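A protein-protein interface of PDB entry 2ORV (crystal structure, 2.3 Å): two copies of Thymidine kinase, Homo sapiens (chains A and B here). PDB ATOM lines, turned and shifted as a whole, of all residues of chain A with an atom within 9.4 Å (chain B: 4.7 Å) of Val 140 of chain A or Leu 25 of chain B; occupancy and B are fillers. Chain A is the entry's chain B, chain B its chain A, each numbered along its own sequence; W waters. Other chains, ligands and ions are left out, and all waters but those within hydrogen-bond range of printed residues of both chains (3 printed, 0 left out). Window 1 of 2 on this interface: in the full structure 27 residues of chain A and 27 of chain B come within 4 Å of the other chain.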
ATOM      1  N   ILE A  21      12.825 -15.858  35.581  1.00  0.00           N
ATOM      2  CA  ILE A  21      13.701 -17.025  35.637  1.00  0.00           C
ATOM      3  C   ILE A  21      14.831 -16.889  34.610  1.00  0.00           C
ATOM      4  O   ILE A  21      14.559 -16.777  33.437  1.00  0.00           O
ATOM      5  CB  ILE A  21      12.926 -18.331  35.363  1.00  0.00           C
ATOM      6  CG1 ILE A  21      11.755 -18.490  36.323  1.00  0.00           C
ATOM      7  CG2 ILE A  21      13.846 -19.553  35.474  1.00  0.00           C
ATOM      8  CD1 ILE A  21      10.909 -19.708  36.048  1.00  0.00           C
ATOM      9  N   GLN A  22      16.084 -16.885  35.054  1.00  0.00           N
ATOM     10  CA  GLN A  22      17.231 -16.884  34.159  1.00  0.00           C
ATOM     11  C   GLN A  22      17.920 -18.252  34.222  1.00  0.00           C
ATOM     12  O   GLN A  22      18.073 -18.792  35.301  1.00  0.00           O
ATOM     13  CB  GLN A  22      18.255 -15.830  34.598  1.00  0.00           C
ATOM     14  CG  GLN A  22      17.707 -14.479  35.061  1.00  0.00           C
ATOM     15  CD  GLN A  22      18.828 -13.526  35.427  1.00  0.00           C
ATOM     16  OE1 GLN A  22      20.053 -13.846  35.331  1.00  0.00           O
ATOM     17  NE2 GLN A  22      18.446 -12.360  35.850  1.00  0.00           N
ATOM     18  N   VAL A  23      18.381 -18.787  33.093  1.00  0.00           N
ATOM     19  CA  VAL A  23      18.961 -20.138  33.078  1.00  0.00           C
ATOM     20  C   VAL A  23      20.363 -20.013  32.523  1.00  0.00           C
ATOM     21  O   VAL A  23      20.575 -19.283  31.560  1.00  0.00           O
ATOM     22  CB  VAL A  23      18.108 -21.171  32.272  1.00  0.00           C
ATOM     23  CG1 VAL A  23      18.680 -22.587  32.377  1.00  0.00           C
ATOM     24  CG2 VAL A  23      16.633 -21.216  32.800  1.00  0.00           C
ATOM     25  N   ILE A  24      21.305 -20.703  33.171  1.00  0.00           N
ATOM     26  CA  ILE A  24      22.705 -20.711  32.794  1.00  0.00           C
ATOM     27  C   ILE A  24      23.144 -22.172  32.557  1.00  0.00           C
ATOM     28  O   ILE A  24      23.284 -22.945  33.499  1.00  0.00           O
ATOM     29  CB  ILE A  24      23.569 -19.990  33.862  1.00  0.00           C
ATOM     30  CG1 ILE A  24      23.056 -18.557  34.104  1.00  0.00           C
ATOM     31  CG2 ILE A  24      25.044 -19.933  33.437  1.00  0.00           C
ATOM     32  CD1 ILE A  24      23.394 -18.036  35.492  1.00  0.00           C
ATOM     33  N   LEU A  25      23.332 -22.550  31.292  1.00  0.00           N
ATOM     34  CA  LEU A  25      23.559 -23.919  30.928  1.00  0.00           C
ATOM     35  C   LEU A  25      25.014 -23.987  30.560  1.00  0.00           C
ATOM     36  O   LEU A  25      25.635 -22.960  30.571  1.00  0.00           O
ATOM     37  CB  LEU A  25      22.672 -24.276  29.749  1.00  0.00           C
ATOM     38  CG  LEU A  25      21.145 -24.257  29.950  1.00  0.00           C
ATOM     39  CD1 LEU A  25      20.430 -24.574  28.685  1.00  0.00           C
ATOM     40  CD2 LEU A  25      20.722 -25.263  31.013  1.00  0.00           C
ATOM     41  N   ILE A 105      12.571 -29.027  40.255  1.00  0.00           N
ATOM     42  CA  ILE A 105      13.022 -27.681  39.818  1.00  0.00           C
ATOM     43  C   ILE A 105      12.085 -26.747  39.006  1.00  0.00           C
ATOM     44  O   ILE A 105      12.039 -25.526  39.249  1.00  0.00           O
ATOM     45  CB  ILE A 105      14.402 -27.789  39.120  1.00  0.00           C
ATOM     46  CG1 ILE A 105      15.041 -26.425  39.017  1.00  0.00           C
ATOM     47  CG2 ILE A 105      14.318 -28.506  37.754  1.00  0.00           C
ATOM     48  CD1 ILE A 105      16.527 -26.432  39.274  1.00  0.00           C
ATOM     49  N   VAL A 106      11.339 -27.321  38.063  1.00  0.00           N
ATOM     50  CA  VAL A 106      10.439 -26.584  37.159  1.00  0.00           C
ATOM     51  C   VAL A 106       9.278 -25.896  37.887  1.00  0.00           C
ATOM     52  O   VAL A 106       9.107 -24.674  37.761  1.00  0.00           O
ATOM     53  CB  VAL A 106       9.951 -27.531  36.008  1.00  0.00           C
ATOM     54  CG1 VAL A 106       8.929 -26.862  35.149  1.00  0.00           C
ATOM     55  CG2 VAL A 106      11.157 -28.014  35.143  1.00  0.00           C
ATOM     56  N   CYS A 109      10.728 -23.186  40.487  1.00  0.00           N
ATOM     57  CA  CYS A 109      11.068 -21.914  39.830  1.00  0.00           C
ATOM     58  C   CYS A 109       9.906 -21.082  39.327  1.00  0.00           C
ATOM     59  O   CYS A 109       9.841 -19.873  39.549  1.00  0.00           O
ATOM     60  CB  CYS A 109      11.990 -22.189  38.674  1.00  0.00           C
ATOM     61  SG  CYS A 109      13.606 -22.638  39.225  1.00  0.00           S
ATOM     62  N   GLU A 110       8.997 -21.745  38.628  1.00  0.00           N
ATOM     63  CA  GLU A 110       7.784 -21.110  38.130  1.00  0.00           C
ATOM     64  C   GLU A 110       6.948 -20.454  39.258  1.00  0.00           C
ATOM     65  O   GLU A 110       6.538 -19.286  39.136  1.00  0.00           O
ATOM     66  CB  GLU A 110       6.987 -22.119  37.278  1.00  0.00           C
ATOM     67  CG  GLU A 110       5.612 -21.654  36.788  1.00  0.00           C
ATOM     68  CD  GLU A 110       5.656 -20.581  35.705  1.00  0.00           C
ATOM     69  OE1 GLU A 110       4.551 -20.181  35.257  1.00  0.00           O
ATOM     70  OE2 GLU A 110       6.762 -20.116  35.315  1.00  0.00           O
ATOM     71  N   VAL A 121      19.289 -19.948  37.648  1.00  0.00           N
ATOM     72  CA  VAL A 121      19.601 -21.381  37.758  1.00  0.00           C
ATOM     73  C   VAL A 121      20.791 -21.766  36.931  1.00  0.00           C
ATOM     74  O   VAL A 121      20.776 -21.550  35.725  1.00  0.00           O
ATOM     75  CB  VAL A 121      18.420 -22.260  37.284  1.00  0.00           C
ATOM     76  CG1 VAL A 121      18.730 -23.708  37.514  1.00  0.00           C
ATOM     77  CG2 VAL A 121      17.115 -21.872  37.971  1.00  0.00           C
ATOM     78  N   ALA A 123      22.872 -25.041  35.672  1.00  0.00           N
ATOM     79  CA  ALA A 123      22.522 -26.452  35.491  1.00  0.00           C
ATOM     80  C   ALA A 123      23.235 -26.916  34.274  1.00  0.00           C
ATOM     81  O   ALA A 123      23.342 -26.161  33.320  1.00  0.00           O
ATOM     82  CB  ALA A 123      21.081 -26.616  35.280  1.00  0.00           C
ATOM     83  N   ASP A 125      23.505 -28.728  30.886  1.00  0.00           N
ATOM     84  CA  ASP A 125      22.456 -29.013  29.901  1.00  0.00           C
ATOM     85  C   ASP A 125      22.351 -30.493  29.528  1.00  0.00           C
ATOM     86  O   ASP A 125      21.246 -31.011  29.356  1.00  0.00           O
ATOM     87  CB  ASP A 125      22.501 -28.102  28.647  1.00  0.00           C
ATOM     88  CG  ASP A 125      23.842 -28.099  27.944  1.00  0.00           C
ATOM     89  OD1 ASP A 125      23.819 -28.225  26.719  1.00  0.00           O
ATOM     90  OD2 ASP A 125      24.915 -27.918  28.576  1.00  0.00           O
ATOM     91  N   ALA A 135      15.287 -32.543  34.651  1.00  0.00           N
ATOM     92  CA  ALA A 135      14.110 -31.801  34.151  1.00  0.00           C
ATOM     93  C   ALA A 135      14.443 -30.366  33.687  1.00  0.00           C
ATOM     94  O   ALA A 135      13.557 -29.574  33.348  1.00  0.00           O
ATOM     95  CB  ALA A 135      13.064 -31.745  35.234  1.00  0.00           C
ATOM     96  N   ILE A 136      15.733 -30.049  33.677  1.00  0.00           N
ATOM     97  CA  ILE A 136      16.215 -28.681  33.503  1.00  0.00           C
ATOM     98  C   ILE A 136      15.768 -27.976  32.205  1.00  0.00           C
ATOM     99  O   ILE A 136      15.462 -26.791  32.219  1.00  0.00           O
ATOM    100  CB  ILE A 136      17.748 -28.644  33.732  1.00  0.00           C
ATOM    101  CG1 ILE A 136      18.029 -27.975  35.074  1.00  0.00           C
ATOM    102  CG2 ILE A 136      18.486 -27.982  32.582  1.00  0.00           C
ATOM    103  CD1 ILE A 136      17.691 -26.495  35.125  1.00  0.00           C
ATOM    104  N   LEU A 137      15.649 -28.705  31.102  1.00  0.00           N
ATOM    105  CA  LEU A 137      15.253 -28.048  29.852  1.00  0.00           C
ATOM    106  C   LEU A 137      13.785 -27.664  29.769  1.00  0.00           C
ATOM    107  O   LEU A 137      13.421 -26.863  28.933  1.00  0.00           O
ATOM    108  CB  LEU A 137      15.718 -28.840  28.604  1.00  0.00           C
ATOM    109  CG  LEU A 137      17.240 -29.070  28.490  1.00  0.00           C
ATOM    110  CD1 LEU A 137      17.600 -29.860  27.246  1.00  0.00           C
ATOM    111  CD2 LEU A 137      18.064 -27.764  28.565  1.00  0.00           C
ATOM    112  N   ASN A 138      12.932 -28.226  30.614  1.00  0.00           N
ATOM    113  CA  ASN A 138      11.549 -27.740  30.684  1.00  0.00           C
ATOM    114  C   ASN A 138      11.486 -26.379  31.328  1.00  0.00           C
ATOM    115  O   ASN A 138      10.446 -25.763  31.322  1.00  0.00           O
ATOM    116  CB  ASN A 138      10.628 -28.692  31.430  1.00  0.00           C
ATOM    117  CG  ASN A 138      10.651 -30.112  30.864  1.00  0.00           C
ATOM    118  OD1 ASN A 138      10.912 -30.324  29.680  1.00  0.00           O
ATOM    119  ND2 ASN A 138      10.363 -31.101  31.724  1.00  0.00           N
ATOM    120  N   LEU A 139      12.602 -25.900  31.872  1.00  0.00           N
ATOM    121  CA  LEU A 139      12.686 -24.509  32.339  1.00  0.00           C
ATOM    122  C   LEU A 139      12.792 -23.485  31.210  1.00  0.00           C
ATOM    123  O   LEU A 139      12.349 -22.340  31.378  1.00  0.00           O
ATOM    124  CB  LEU A 139      13.872 -24.315  33.259  1.00  0.00           C
ATOM    125  CG  LEU A 139      13.860 -24.526  34.777  1.00  0.00           C
ATOM    126  CD1 LEU A 139      15.204 -24.055  35.297  1.00  0.00           C
ATOM    127  CD2 LEU A 139      12.748 -23.762  35.436  1.00  0.00           C
ATOM    128  N   VAL A 140      13.371 -23.890  30.071  1.00  0.00           N
ATOM    129  CA  VAL A 140      13.546 -22.999  28.902  1.00  0.00           C
ATOM    130  C   VAL A 140      12.290 -22.241  28.406  1.00  0.00           C
ATOM    131  O   VAL A 140      12.323 -21.015  28.296  1.00  0.00           O
ATOM    132  CB  VAL A 140      14.252 -23.724  27.724  1.00  0.00           C
ATOM    133  CG1 VAL A 140      14.538 -22.728  26.574  1.00  0.00           C
ATOM    134  CG2 VAL A 140      15.535 -24.369  28.201  1.00  0.00           C
ATOM    135  N   PRO A 141      11.181 -22.955  28.096  1.00  0.00           N
ATOM    136  CA  PRO A 141       9.961 -22.240  27.717  1.00  0.00           C
ATOM    137  C   PRO A 141       9.418 -21.249  28.749  1.00  0.00           C
ATOM    138  O   PRO A 141       8.602 -20.363  28.400  1.00  0.00           O
ATOM    139  CB  PRO A 141       8.946 -23.378  27.492  1.00  0.00           C
ATOM    140  CG  PRO A 141       9.795 -24.581  27.196  1.00  0.00           C
ATOM    141  CD  PRO A 141      11.004 -24.419  28.017  1.00  0.00           C
ATOM    142  N   LEU A 142       9.854 -21.369  30.000  1.00  0.00           N
ATOM    143  CA  LEU A 142       9.317 -20.525  31.097  1.00  0.00           C
ATOM    144  C   LEU A 142      10.274 -19.385  31.460  1.00  0.00           C
ATOM    145  O   LEU A 142       9.878 -18.400  32.099  1.00  0.00           O
ATOM    146  CB  LEU A 142       9.078 -21.369  32.343  1.00  0.00           C
ATOM    147  CG  LEU A 142       8.460 -22.762  32.214  1.00  0.00           C
ATOM    148  CD1 LEU A 142       8.783 -23.528  33.446  1.00  0.00           C
ATOM    149  CD2 LEU A 142       6.963 -22.626  32.075  1.00  0.00           C
ATOM    150  N   ALA A 143      11.541 -19.555  31.069  1.00  0.00           N
ATOM    151  CA  ALA A 143      12.609 -18.624  31.383  1.00  0.00           C
ATOM    152  C   ALA A 143      12.574 -17.347  30.542  1.00  0.00           C
ATOM    153  O   ALA A 143      12.261 -17.370  29.351  1.00  0.00           O
ATOM    154  CB  ALA A 143      13.968 -19.311  31.264  1.00  0.00           C
ATOM    155  N   GLU A 144      12.902 -16.231  31.183  1.00  0.00           N
ATOM    156  CA  GLU A 144      13.058 -14.960  30.513  1.00  0.00           C
ATOM    157  C   GLU A 144      14.398 -14.889  29.823  1.00  0.00           C
ATOM    158  O   GLU A 144      14.549 -14.194  28.808  1.00  0.00           O
ATOM    159  CB  GLU A 144      12.934 -13.821  31.500  1.00  0.00           C
ATOM    160  CG  GLU A 144      11.483 -13.347  31.706  1.00  0.00           C
ATOM    161  CD  GLU A 144      10.678 -14.107  32.776  1.00  0.00           C
ATOM    162  OE1 GLU A 144      10.975 -15.298  33.117  1.00  0.00           O
ATOM    163  OE2 GLU A 144       9.678 -13.507  33.234  1.00  0.00           O
ATOM    164  N   SER A 145      15.401 -15.567  30.358  1.00  0.00           N
ATOM    165  CA  SER A 145      16.682 -15.563  29.651  1.00  0.00           C
ATOM    166  C   SER A 145      17.390 -16.888  29.714  1.00  0.00           C
ATOM    167  O   SER A 145      17.331 -17.580  30.719  1.00  0.00           O
ATOM    168  CB  SER A 145      17.591 -14.432  30.141  1.00  0.00           C
ATOM    169  OG  SER A 145      18.309 -14.826  31.275  1.00  0.00           O
ATOM    170  N   VAL A 146      18.083 -17.219  28.636  1.00  0.00           N
ATOM    171  CA  VAL A 146      18.790 -18.482  28.553  1.00  0.00           C
ATOM    172  C   VAL A 146      20.112 -18.234  27.852  1.00  0.00           C
ATOM    173  O   VAL A 146      20.169 -17.551  26.809  1.00  0.00           O
ATOM    174  CB  VAL A 146      17.969 -19.578  27.793  1.00  0.00           C
ATOM    175  CG1 VAL A 146      18.691 -20.893  27.810  1.00  0.00           C
ATOM    176  CG2 VAL A 146      16.550 -19.720  28.386  1.00  0.00           C
ATOM    177  N   VAL A 147      21.180 -18.791  28.435  1.00  0.00           N
ATOM    178  CA  VAL A 147      22.521 -18.701  27.853  1.00  0.00           C
ATOM    179  C   VAL A 147      23.202 -20.052  28.038  1.00  0.00           C
ATOM    180  O   VAL A 147      22.866 -20.750  28.963  1.00  0.00           O
ATOM    181  CB  VAL A 147      23.307 -17.530  28.501  1.00  0.00           C
ATOM    182  CG1 VAL A 147      23.901 -17.891  29.899  1.00  0.00           C
ATOM    183  CG2 VAL A 147      24.386 -17.057  27.570  1.00  0.00           C
ATOM    184  N   LYS A 148      24.147 -20.424  27.180  1.00  0.00           N
ATOM    185  CA  LYS A 148      24.899 -21.635  27.417  1.00  0.00           C
ATOM    186  C   LYS A 148      26.397 -21.301  27.350  1.00  0.00           C
ATOM    187  O   LYS A 148      26.865 -20.862  26.319  1.00  0.00           O
ATOM    188  CB  LYS A 148      24.526 -22.709  26.389  1.00  0.00           C
ATOM    189  CG  LYS A 148      25.596 -23.797  26.195  1.00  0.00           C
ATOM    190  CD  LYS A 148      25.025 -25.121  25.636  1.00  0.00           C
ATOM    191  CE  LYS A 148      26.083 -26.232  25.637  1.00  0.00           C
ATOM    192  NZ  LYS A 148      25.611 -27.456  24.850  1.00  0.00           N
ATOM    193  N   VAL B  23      21.900 -22.599  18.075  1.00  0.00           N
ATOM    194  CA  VAL B  23      20.421 -22.599  18.222  1.00  0.00           C
ATOM    195  C   VAL B  23      19.984 -21.200  18.646  1.00  0.00           C
ATOM    196  O   VAL B  23      20.536 -20.653  19.592  1.00  0.00           O
ATOM    197  CB  VAL B  23      19.942 -23.585  19.331  1.00  0.00           C
ATOM    198  CG1 VAL B  23      18.458 -23.414  19.638  1.00  0.00           C
ATOM    199  CG2 VAL B  23      20.241 -24.994  18.992  1.00  0.00           C
ATOM    200  N   ILE B  24      18.967 -20.660  17.971  1.00  0.00           N
ATOM    201  CA  ILE B  24      18.410 -19.347  18.269  1.00  0.00           C
ATOM    202  C   ILE B  24      16.960 -19.514  18.690  1.00  0.00           C
ATOM    203  O   ILE B  24      16.127 -19.794  17.859  1.00  0.00           O
ATOM    204  CB  ILE B  24      18.486 -18.408  17.061  1.00  0.00           C
ATOM    205  CG1 ILE B  24      19.947 -18.277  16.601  1.00  0.00           C
ATOM    206  CG2 ILE B  24      17.937 -16.982  17.416  1.00  0.00           C
ATOM    207  CD1 ILE B  24      20.056 -17.813  15.156  1.00  0.00           C
ATOM    208  N   LEU B  25      16.680 -19.366  19.984  1.00  0.00           N
ATOM    209  CA  LEU B  25      15.313 -19.441  20.527  1.00  0.00           C
ATOM    210  C   LEU B  25      14.750 -18.077  20.818  1.00  0.00           C
ATOM    211  O   LEU B  25      15.450 -17.091  20.739  1.00  0.00           O
ATOM    212  CB  LEU B  25      15.304 -20.261  21.821  1.00  0.00           C
ATOM    213  CG  LEU B  25      16.135 -21.537  21.792  1.00  0.00           C
ATOM    214  CD1 LEU B  25      16.408 -22.038  23.211  1.00  0.00           C
ATOM    215  CD2 LEU B  25      15.465 -22.649  20.933  1.00  0.00           C
ATOM    216  N   GLY B  26      13.477 -18.026  21.172  1.00  0.00           N
ATOM    217  CA  GLY B  26      12.828 -16.770  21.403  1.00  0.00           C
ATOM    218  C   GLY B  26      11.314 -16.894  21.288  1.00  0.00           C
ATOM    219  O   GLY B  26      10.803 -17.879  20.735  1.00  0.00           O
ATOM    220  N   LYS B  32      14.177 -13.929  15.282  1.00  0.00           N
ATOM    221  CA  LYS B  32      14.979 -15.168  15.154  1.00  0.00           C
ATOM    222  C   LYS B  32      15.468 -15.460  13.754  1.00  0.00           C
ATOM    223  O   LYS B  32      16.565 -16.016  13.581  1.00  0.00           O
ATOM    224  CB  LYS B  32      14.228 -16.388  15.704  1.00  0.00           C
ATOM    225  CG  LYS B  32      13.509 -16.137  17.102  1.00  0.00           C
ATOM    226  CD  LYS B  32      12.779 -17.391  17.576  1.00  0.00           C
ATOM    227  CE  LYS B  32      11.532 -17.652  16.742  1.00  0.00           C
ATOM    228  NZ  LYS B  32      10.595 -16.510  16.979  1.00  0.00           N
ATOM    229  N   ALA B 123      14.202 -21.115  16.001  1.00  0.00           N
ATOM    230  CA  ALA B 123      13.049 -21.888  16.480  1.00  0.00           C
ATOM    231  C   ALA B 123      12.484 -21.243  17.737  1.00  0.00           C
ATOM    232  O   ALA B 123      13.207 -20.681  18.550  1.00  0.00           O
ATOM    233  CB  ALA B 123      13.451 -23.326  16.803  1.00  0.00           C
ATOM    234  N   ASP B 125      10.992 -21.697  21.334  1.00  0.00           N
ATOM    235  CA  ASP B 125      11.215 -22.622  22.444  1.00  0.00           C
ATOM    236  C   ASP B 125       9.910 -23.164  23.074  1.00  0.00           C
ATOM    237  O   ASP B 125       9.832 -24.361  23.415  1.00  0.00           O
ATOM    238  CB  ASP B 125      12.120 -21.967  23.498  1.00  0.00           C
ATOM    239  CG  ASP B 125      11.596 -20.648  23.948  1.00  0.00           C
ATOM    240  OD1 ASP B 125      11.748 -20.349  25.137  1.00  0.00           O
ATOM    241  OD2 ASP B 125      10.992 -19.915  23.132  1.00  0.00           O
ATOM    242  N   ILE B 136      12.566 -29.599  19.734  1.00  0.00           N
ATOM    243  CA  ILE B 136      13.606 -28.610  19.511  1.00  0.00           C
ATOM    244  C   ILE B 136      14.561 -28.553  20.717  1.00  0.00           C
ATOM    245  O   ILE B 136      15.779 -28.389  20.544  1.00  0.00           O
ATOM    246  CB  ILE B 136      12.971 -27.257  19.039  1.00  0.00           C
ATOM    247  CG1 ILE B 136      13.661 -26.716  17.780  1.00  0.00           C
ATOM    248  CG2 ILE B 136      12.694 -26.307  20.194  1.00  0.00           C
ATOM    249  CD1 ILE B 136      15.146 -26.438  17.897  1.00  0.00           C
ATOM    250  N   LEU B 137      14.021 -28.793  21.917  1.00  0.00           N
ATOM    251  CA  LEU B 137      14.845 -28.716  23.122  1.00  0.00           C
ATOM    252  C   LEU B 137      15.893 -29.812  23.252  1.00  0.00           C
ATOM    253  O   LEU B 137      16.861 -29.659  24.014  1.00  0.00           O
ATOM    254  CB  LEU B 137      14.022 -28.562  24.404  1.00  0.00           C
ATOM    255  CG  LEU B 137      13.159 -27.287  24.475  1.00  0.00           C
ATOM    256  CD1 LEU B 137      12.590 -27.185  25.867  1.00  0.00           C
ATOM    257  CD2 LEU B 137      13.841 -25.951  24.080  1.00  0.00           C
ATOM    258  N   VAL B 146      23.719 -21.659  22.375  1.00  0.00           N
ATOM    259  CA  VAL B 146      22.273 -21.483  22.556  1.00  0.00           C
ATOM    260  C   VAL B 146      22.029 -20.072  23.056  1.00  0.00           C
ATOM    261  O   VAL B 146      22.615 -19.639  24.049  1.00  0.00           O
ATOM    262  CB  VAL B 146      21.640 -22.517  23.541  1.00  0.00           C
ATOM    263  CG1 VAL B 146      20.091 -22.339  23.643  1.00  0.00           C
ATOM    264  CG2 VAL B 146      22.042 -23.965  23.166  1.00  0.00           C
ATOM    265  N   VAL B 147      21.209 -19.323  22.320  1.00  0.00           N
ATOM    266  CA  VAL B 147      20.728 -18.043  22.826  1.00  0.00           C
ATOM    267  C   VAL B 147      19.207 -18.010  22.816  1.00  0.00           C
ATOM    268  O   VAL B 147      18.581 -18.726  21.986  1.00  0.00           O
ATOM    269  CB  VAL B 147      21.352 -16.813  22.071  1.00  0.00           C
ATOM    270  CG1 VAL B 147      20.772 -16.610  20.670  1.00  0.00           C
ATOM    271  CG2 VAL B 147      21.183 -15.576  22.910  1.00  0.00           C
ATOM    272  N   LYS B 148      18.634 -17.218  23.736  1.00  0.00           N
ATOM    273  CA  LYS B 148      17.216 -16.904  23.696  1.00  0.00           C
ATOM    274  C   LYS B 148      16.949 -15.411  23.509  1.00  0.00           C
ATOM    275  O   LYS B 148      17.362 -14.591  24.304  1.00  0.00           O
ATOM    276  CB  LYS B 148      16.463 -17.435  24.905  1.00  0.00           C
ATOM    277  CG  LYS B 148      15.042 -16.988  24.957  1.00  0.00           C
ATOM    278  CD  LYS B 148      14.147 -18.031  25.698  1.00  0.00           C
ATOM    279  CE  LYS B 148      12.744 -17.471  25.897  1.00  0.00           C
ATOM    280  NZ  LYS B 148      11.785 -18.352  26.677  1.00  0.00           N
ATOM    281  N   LEU B 149      16.254 -15.077  22.432  1.00  0.00           N
ATOM    282  CA  LEU B 149      16.005 -13.708  22.065  1.00  0.00           C
ATOM    283  C   LEU B 149      14.806 -13.093  22.824  1.00  0.00           C
ATOM    284  O   LEU B 149      14.120 -13.744  23.607  1.00  0.00           O
ATOM    285  CB  LEU B 149      15.891 -13.592  20.545  1.00  0.00           C
ATOM    286  CG  LEU B 149      17.240 -13.911  19.858  1.00  0.00           C
ATOM    287  CD1 LEU B 149      17.080 -14.025  18.338  1.00  0.00           C
ATOM    288  CD2 LEU B 149      18.376 -12.874  20.244  1.00  0.00           C
HETATM  289  O   HOH W   1      18.823 -15.116  26.845  1.00  0.00           O
HETATM  290  O   HOH W   2      12.968 -13.537  26.131  1.00  0.00           O
HETATM  291  O   HOH W   3      25.808 -19.905  23.620  1.00  0.00           O
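Leu 25 of chain A touches none of the printed residues of chain B.
Of the printed residues of chain B, Leu 137 of chain A touches Leu 137.
Of chain B, only Leu 25 (3.9 Å), Asp 125 (3.3 Å) and Lys 148 (3.2 Å) come within 4 Å of Val 140 of chain A.
Of the printed residues of chain B, Val 146 of chain A touches Lys 148 (3.5 Å).
Printed residues of chain B within 4 Å of Lys 148 of chain A: Val 146 (3.6 Å).
Of chain A, only Val 140 comes within 4 Å of Leu 25 of chain B.
No residue of chain A comes within 4 Å of Gly 26 of chain B.
Printed residues of chain A within 4 Å of Asp 125 of chain B: Val 140 and Pro 141.
Of the printed residues of chain A, Val 146 of chain B touches Val 147 (3.9 Å) and Lys 148 (3.6 Å).
No residue of chain A comes within 4 Å of Leu 149 of chain B.
The nearest printed residue of chain B that does not touch Lys 148 of chain A is Val 147 of chain B (5.8 Å).
Water W2 lies within hydrogen-bond range of the backbone carbonyl oxygen of Leu 149 of chain B (2.8 Å) and the backbone carbonyl oxygen of Glu 144 of chain A (3.2 Å).
Water W1 lies within hydrogen-bond range of O of Val 146 of chain A (2.8 Å) and O of Lys 148 of chain B (3.0 Å).
Water W3 lies within hydrogen-bond range of the backbone NH (N) of Val 146 of chain B (3.0 Å) and the backbone carbonyl oxygen (O) of Lys 148 of chain A (3.1 Å).
O of Leu 25 of chain B is in hydrogen-bond range of N of Leu 149 of chain B, 2.8 Å away.
The side-chain amino group (NZ) of Lys 148 of chain B is in salt-bridge range of the side-chain carboxylate (OD1) of Asp 125 of chain B, 2.5 Å away.
The backbone NH of Leu 25 of chain A is in hydrogen-bond range of the backbone carbonyl oxygen of Val 147 of chain A, at 3.0 Å.
The side-chain amino group (NZ) of Lys 148 of chain A lies within salt-bridge range of the side-chain carboxylate (OD1) of Asp 125 of chain A (2.7 Å).
N of Val 147 of chain A lies within hydrogen-bond range of O of Val 23 of chain A, at 3.2 Å.
O of Val 147 of chain B sits at hydrogen-bond distance from N of Leu 25 of chain B (2.8 Å).
Leu 137 of chain A touches its own counterpart, Leu 137 of chain B.
Val 146 of chain A touches Lys 148 of chain B, and with the chains exchanged Lys 148 of chain A touches Val 146 of chain B.
Val 147 of chain A touches Val 146 of chain B, but with the chains exchanged Val 146 of chain A does not touch Val 147 of chain B (4.1 Å).
Of the 10 pairs that touch across the chains among the printed residues, 3 have their exchanged pair printed and touching as well.
Among the printed residues, pairs that only touch across the chains: Leu 137 of chain A with Leu 137 of chain B (3.2 Å), Lys 148 of chain A with Val 146 of chain B (3.6 Å), Pro 141 of chain A with Asp 125 of chain B (3.7 Å), Pro 141 of chain A with Leu 137 of chain B (3.8 Å), Val 140 of chain A with Leu 25 of chain B (3.9 Å) and Val 147 of chain A with Val 146 of chain B (3.9 Å).
Of the 26 printed residues of chain A, 7 touch a printed residue of chain B.
Hydrophobic or aromatic side chains of chain B that line the printed part of chain A: Leu 25 and Leu 137.
Along chain B the printed residues that touch a printed residue of chain A span positions 25 to 148.
The backbone NH (N) of Lys 148 of chain B sits at hydrogen-bond distance from the backbone carbonyl oxygen (O) of Val 146 of chain A (3.5 Å).
O of Val 140 of chain A lies close to OD1 of Asp 125 of chain B, at 3.3 Å.
The side-chain amino group of Lys 148 of chain B is in hydrogen-bond range of the backbone carbonyl oxygen of Val 140 of chain A (3.2 Å).
O of Ala 143 of chain A sits at hydrogen-bond distance from NZ of Lys 148 of chain B.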
